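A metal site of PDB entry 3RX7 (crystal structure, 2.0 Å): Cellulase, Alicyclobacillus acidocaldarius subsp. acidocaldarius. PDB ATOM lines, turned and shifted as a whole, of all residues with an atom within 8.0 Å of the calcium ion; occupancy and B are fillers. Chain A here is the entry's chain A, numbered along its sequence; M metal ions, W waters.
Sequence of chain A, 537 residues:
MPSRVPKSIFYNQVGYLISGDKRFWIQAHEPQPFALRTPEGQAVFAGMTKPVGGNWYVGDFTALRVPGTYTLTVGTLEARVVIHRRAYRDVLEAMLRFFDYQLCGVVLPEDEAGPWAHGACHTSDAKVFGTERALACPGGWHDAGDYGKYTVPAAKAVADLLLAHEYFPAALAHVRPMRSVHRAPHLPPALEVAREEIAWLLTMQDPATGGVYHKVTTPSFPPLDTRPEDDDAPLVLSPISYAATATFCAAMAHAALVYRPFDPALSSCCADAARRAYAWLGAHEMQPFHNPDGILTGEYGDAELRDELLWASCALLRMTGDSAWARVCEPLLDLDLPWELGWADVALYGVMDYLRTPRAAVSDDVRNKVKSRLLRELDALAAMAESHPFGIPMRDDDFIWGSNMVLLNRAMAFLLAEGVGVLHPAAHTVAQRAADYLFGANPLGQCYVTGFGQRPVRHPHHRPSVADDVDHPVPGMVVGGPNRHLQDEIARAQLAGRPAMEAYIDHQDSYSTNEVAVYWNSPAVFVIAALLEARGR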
ATOM      1  N   VAL A 152      11.305 -23.767  11.026  1.00  0.00           N
ATOM      2  CA  VAL A 152      11.603 -24.048   9.631  1.00  0.00           C
ATOM      3  C   VAL A 152      13.054 -24.491   9.417  1.00  0.00           C
ATOM      4  O   VAL A 152      13.249 -25.619   8.984  1.00  0.00           O
ATOM      5  CB  VAL A 152      11.085 -22.936   8.667  1.00  0.00           C
ATOM      6  CG1 VAL A 152      11.678 -23.063   7.276  1.00  0.00           C
ATOM      7  CG2 VAL A 152       9.570 -22.949   8.626  1.00  0.00           C
ATOM      8  N   ALA A 243       4.317 -23.130   6.903  1.00  0.00           N
ATOM      9  CA  ALA A 243       5.680 -23.600   6.661  1.00  0.00           C
ATOM     10  C   ALA A 243       6.252 -24.336   7.870  1.00  0.00           C
ATOM     11  O   ALA A 243       6.831 -25.406   7.689  1.00  0.00           O
ATOM     12  CB  ALA A 243       6.559 -22.445   6.261  1.00  0.00           C
ATOM     13  N   THR A 247       7.124 -28.313   7.642  1.00  0.00           N
ATOM     14  CA  THR A 247       8.527 -28.743   7.815  1.00  0.00           C
ATOM     15  C   THR A 247       8.679 -29.620   9.078  1.00  0.00           C
ATOM     16  O   THR A 247       9.420 -30.597   9.062  1.00  0.00           O
ATOM     17  CB  THR A 247       9.507 -27.579   7.794  1.00  0.00           C
ATOM     18  OG1 THR A 247       9.162 -26.676   8.830  1.00  0.00           O
ATOM     19  CG2 THR A 247       9.559 -26.886   6.430  1.00  0.00           C
ATOM     20  N   GLY A 301      10.677 -16.287   6.404  1.00  0.00           N
ATOM     21  CA  GLY A 301       9.494 -16.155   5.590  1.00  0.00           C
ATOM     22  C   GLY A 301       9.703 -16.900   4.288  1.00  0.00           C
ATOM     23  O   GLY A 301      10.833 -17.242   3.948  1.00  0.00           O
ATOM     24  N   ASP A 302       8.620 -17.138   3.550  1.00  0.00           N
ATOM     25  CA  ASP A 302       8.669 -17.884   2.283  1.00  0.00           C
ATOM     26  C   ASP A 302       7.314 -17.832   1.618  1.00  0.00           C
ATOM     27  O   ASP A 302       6.328 -18.233   2.226  1.00  0.00           O
ATOM     28  CB  ASP A 302       9.070 -19.345   2.574  1.00  0.00           C
ATOM     29  CG  ASP A 302       9.208 -20.277   1.401  1.00  0.00           C
ATOM     30  OD1 ASP A 302       9.448 -19.784   0.257  1.00  0.00           O
ATOM     31  OD2 ASP A 302       9.103 -21.501   1.609  1.00  0.00           O
ATOM     32  N   ALA A 303       7.257 -17.330   0.364  1.00  0.00           N
ATOM     33  CA  ALA A 303       5.987 -17.230  -0.367  1.00  0.00           C
ATOM     34  C   ALA A 303       5.541 -18.545  -1.006  1.00  0.00           C
ATOM     35  O   ALA A 303       4.348 -18.699  -1.308  1.00  0.00           O
ATOM     36  CB  ALA A 303       6.066 -16.147  -1.436  1.00  0.00           C
ATOM     37  N   GLU A 304       6.490 -19.501  -1.217  1.00  0.00           N
ATOM     38  CA  GLU A 304       6.193 -20.786  -1.887  1.00  0.00           C
ATOM     39  C   GLU A 304       6.138 -21.925  -0.904  1.00  0.00           C
ATOM     40  O   GLU A 304       7.181 -22.322  -0.341  1.00  0.00           O
ATOM     41  CB  GLU A 304       7.185 -21.067  -3.033  1.00  0.00           C
ATOM     42  CG  GLU A 304       6.939 -22.394  -3.749  1.00  0.00           C
ATOM     43  CD  GLU A 304       5.563 -22.518  -4.372  1.00  0.00           C
ATOM     44  OE1 GLU A 304       5.275 -21.793  -5.353  1.00  0.00           O
ATOM     45  OE2 GLU A 304       4.724 -23.252  -3.786  1.00  0.00           O
ATOM     46  N   LEU A 305       4.934 -22.492  -0.743  1.00  0.00           N
ATOM     47  CA  LEU A 305       4.681 -23.516   0.248  1.00  0.00           C
ATOM     48  C   LEU A 305       4.362 -24.895  -0.285  1.00  0.00           C
ATOM     49  O   LEU A 305       4.171 -25.829   0.506  1.00  0.00           O
ATOM     50  CB  LEU A 305       3.652 -23.025   1.284  1.00  0.00           C
ATOM     51  CG  LEU A 305       4.007 -21.690   2.037  1.00  0.00           C
ATOM     52  CD1 LEU A 305       2.822 -21.186   2.859  1.00  0.00           C
ATOM     53  CD2 LEU A 305       5.225 -21.841   2.943  1.00  0.00           C
ATOM     54  N   ARG A 306       4.357 -25.050  -1.623  1.00  0.00           N
ATOM     55  CA  ARG A 306       4.060 -26.361  -2.211  1.00  0.00           C
ATOM     56  C   ARG A 306       5.161 -27.362  -1.991  1.00  0.00           C
ATOM     57  O   ARG A 306       4.877 -28.538  -1.817  1.00  0.00           O
ATOM     58  CB  ARG A 306       3.653 -26.236  -3.675  1.00  0.00           C
ATOM     59  CG  ARG A 306       2.285 -25.555  -3.793  1.00  0.00           C
ATOM     60  CD  ARG A 306       1.941 -25.160  -5.197  1.00  0.00           C
ATOM     61  NE  ARG A 306       2.906 -24.181  -5.701  1.00  0.00           N
ATOM     62  CZ  ARG A 306       2.996 -23.838  -6.977  1.00  0.00           C
ATOM     63  NH1 ARG A 306       2.189 -24.373  -7.870  1.00  0.00           N
ATOM     64  NH2 ARG A 306       3.915 -22.955  -7.356  1.00  0.00           N
ATOM     65  N   ASP A 307       6.415 -26.889  -1.965  1.00  0.00           N
ATOM     66  CA  ASP A 307       7.557 -27.746  -1.727  1.00  0.00           C
ATOM     67  C   ASP A 307       7.535 -28.313  -0.291  1.00  0.00           C
ATOM     68  O   ASP A 307       7.895 -29.476  -0.103  1.00  0.00           O
ATOM     69  CB  ASP A 307       8.864 -27.004  -2.045  1.00  0.00           C
ATOM     70  CG  ASP A 307       9.021 -25.665  -1.343  1.00  0.00           C
ATOM     71  OD1 ASP A 307       8.250 -24.720  -1.653  1.00  0.00           O
ATOM     72  OD2 ASP A 307       9.979 -25.523  -0.560  1.00  0.00           O
ATOM     73  N   GLU A 308       7.051 -27.521   0.712  1.00  0.00           N
ATOM     74  CA  GLU A 308       6.923 -27.961   2.098  1.00  0.00           C
ATOM     75  C   GLU A 308       5.828 -29.039   2.173  1.00  0.00           C
ATOM     76  O   GLU A 308       5.992 -30.026   2.885  1.00  0.00           O
ATOM     77  CB  GLU A 308       6.575 -26.786   3.041  1.00  0.00           C
ATOM     78  CG  GLU A 308       7.739 -25.844   3.358  1.00  0.00           C
ATOM     79  CD  GLU A 308       8.188 -24.890   2.261  1.00  0.00           C
ATOM     80  OE1 GLU A 308       7.426 -24.684   1.291  1.00  0.00           O
ATOM     81  OE2 GLU A 308       9.335 -24.410   2.323  1.00  0.00           O
ATOM     82  N   LEU A 309       4.700 -28.863   1.428  1.00  0.00           N
ATOM     83  CA  LEU A 309       3.639 -29.874   1.408  1.00  0.00           C
ATOM     84  C   LEU A 309       4.159 -31.145   0.723  1.00  0.00           C
ATOM     85  O   LEU A 309       3.849 -32.243   1.183  1.00  0.00           O
ATOM     86  CB  LEU A 309       2.390 -29.354   0.677  1.00  0.00           C
ATOM     87  CG  LEU A 309       1.180 -30.309   0.580  1.00  0.00           C
ATOM     88  CD1 LEU A 309       0.683 -30.760   1.971  1.00  0.00           C
ATOM     89  CD2 LEU A 309       0.050 -29.679  -0.279  1.00  0.00           C
ATOM     90  N   LEU A 337       8.818 -26.838  -9.345  1.00  0.00           N
ATOM     91  CA  LEU A 337       9.458 -26.325  -8.150  1.00  0.00           C
ATOM     92  C   LEU A 337      10.978 -26.596  -8.237  1.00  0.00           C
ATOM     93  O   LEU A 337      11.378 -27.645  -8.743  1.00  0.00           O
ATOM     94  CB  LEU A 337       8.886 -27.044  -6.903  1.00  0.00           C
ATOM     95  CG  LEU A 337       7.421 -26.800  -6.543  1.00  0.00           C
ATOM     96  CD1 LEU A 337       6.912 -27.858  -5.589  1.00  0.00           C
ATOM     97  CD2 LEU A 337       7.237 -25.422  -5.899  1.00  0.00           C
ATOM     98  N   PRO A 338      11.850 -25.708  -7.712  1.00  0.00           N
ATOM     99  CA  PRO A 338      13.276 -26.069  -7.674  1.00  0.00           C
ATOM    100  C   PRO A 338      13.443 -27.241  -6.682  1.00  0.00           C
ATOM    101  O   PRO A 338      12.728 -27.306  -5.685  1.00  0.00           O
ATOM    102  CB  PRO A 338      13.942 -24.798  -7.131  1.00  0.00           C
ATOM    103  CG  PRO A 338      12.849 -24.058  -6.407  1.00  0.00           C
ATOM    104  CD  PRO A 338      11.574 -24.403  -7.075  1.00  0.00           C
ATOM    105  N   GLY A 342      16.716 -26.811   1.002  1.00  0.00           N
ATOM    106  CA  GLY A 342      16.364 -25.814   2.003  1.00  0.00           C
ATOM    107  C   GLY A 342      17.284 -24.612   2.156  1.00  0.00           C
ATOM    108  O   GLY A 342      18.183 -24.443   1.341  1.00  0.00           O
ATOM    109  N   TRP A 343      17.059 -23.738   3.166  1.00  0.00           N
ATOM    110  CA  TRP A 343      16.004 -23.844   4.180  1.00  0.00           C
ATOM    111  C   TRP A 343      14.593 -23.516   3.650  1.00  0.00           C
ATOM    112  O   TRP A 343      13.607 -23.998   4.209  1.00  0.00           O
ATOM    113  CB  TRP A 343      16.351 -22.982   5.430  1.00  0.00           C
ATOM    114  CG  TRP A 343      16.439 -21.497   5.143  1.00  0.00           C
ATOM    115  CD1 TRP A 343      17.572 -20.790   4.877  1.00  0.00           C
ATOM    116  CD2 TRP A 343      15.354 -20.562   5.077  1.00  0.00           C
ATOM    117  NE1 TRP A 343      17.262 -19.472   4.638  1.00  0.00           N
ATOM    118  CE2 TRP A 343      15.901 -19.302   4.760  1.00  0.00           C
ATOM    119  CE3 TRP A 343      13.954 -20.673   5.205  1.00  0.00           C
ATOM    120  CZ2 TRP A 343      15.107 -18.144   4.596  1.00  0.00           C
ATOM    121  CZ3 TRP A 343      13.165 -19.532   5.033  1.00  0.00           C
ATOM    122  CH2 TRP A 343      13.747 -18.291   4.731  1.00  0.00           C
ATOM    123  N   ALA A 344      14.487 -22.663   2.597  1.00  0.00           N
ATOM    124  CA  ALA A 344      13.220 -22.224   2.030  1.00  0.00           C
ATOM    125  C   ALA A 344      12.631 -23.134   0.935  1.00  0.00           C
ATOM    126  O   ALA A 344      11.412 -23.244   0.818  1.00  0.00           O
ATOM    127  CB  ALA A 344      13.347 -20.785   1.520  1.00  0.00           C
ATOM    128  N   ASP A 345      13.487 -23.719   0.102  1.00  0.00           N
ATOM    129  CA  ASP A 345      13.109 -24.566  -1.028  1.00  0.00           C
ATOM    130  C   ASP A 345      13.582 -25.960  -0.656  1.00  0.00           C
ATOM    131  O   ASP A 345      14.755 -26.267  -0.743  1.00  0.00           O
ATOM    132  CB  ASP A 345      13.800 -24.024  -2.304  1.00  0.00           C
ATOM    133  CG  ASP A 345      13.481 -22.566  -2.551  1.00  0.00           C
ATOM    134  OD1 ASP A 345      14.360 -21.711  -2.299  1.00  0.00           O
ATOM    135  OD2 ASP A 345      12.307 -22.259  -2.917  1.00  0.00           O
ATOM    136  N   VAL A 346      12.657 -26.774  -0.184  1.00  0.00           N
ATOM    137  CA  VAL A 346      12.902 -28.095   0.388  1.00  0.00           C
ATOM    138  C   VAL A 346      12.448 -29.287  -0.447  1.00  0.00           C
ATOM    139  O   VAL A 346      12.437 -30.399   0.085  1.00  0.00           O
ATOM    140  CB  VAL A 346      12.251 -28.147   1.803  1.00  0.00           C
ATOM    141  CG1 VAL A 346      12.770 -27.025   2.712  1.00  0.00           C
ATOM    142  CG2 VAL A 346      10.720 -28.101   1.720  1.00  0.00           C
ATOM    143  N   ALA A 347      12.015 -29.081  -1.704  1.00  0.00           N
ATOM    144  CA  ALA A 347      11.476 -30.174  -2.516  1.00  0.00           C
ATOM    145  C   ALA A 347      12.376 -31.423  -2.652  1.00  0.00           C
ATOM    146  O   ALA A 347      11.849 -32.537  -2.637  1.00  0.00           O
ATOM    147  CB  ALA A 347      11.004 -29.664  -3.862  1.00  0.00           C
HETATM  148 CA    CA M   1       9.121 -23.403   0.234  1.00  0.00          CA
HETATM  149  O   HOH W   1       9.995 -21.934  -1.298  1.00  0.00           O
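Five residues have an atom within 4 Å of the calcium ion: Asp 302, Glu 304, Asp 307, Glu 308 and Ala 344.
Along chain A the residues within 4 Å of the calcium ion span positions 302 to 344.
O of Glu 304 binds the calcium ion, at 2.3 Å.
The calcium ion is bound by water W1 (2.3 Å).
The calcium ion is bound by OE2 of Glu 308 (2.3 Å).
The side-chain carboxylate (OD2) of Asp 302 is bound to the calcium ion (2.3 Å).
O of Ala 344 binds the calcium ion, 2.4 Å away.
The side-chain carboxylate (OE1) of Glu 308 is bound to the calcium ion (2.4 Å).
The calcium ion is bound by OD2 of Asp 307 (2.4 Å).
OD1 of Asp 307 is bound to the calcium ion (2.5 Å).
The guanidinium group (NH2) of Arg 306 is in salt-bridge range of the side-chain carboxylate (OE1) of Glu 304.
The backbone NH of Val 346 lies close to the side-chain carboxylate of Asp 307 (3.0 Å).
Water W1 lies within hydrogen-bond range of OD1 of Asp 302 and OD2 of Asp 345.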
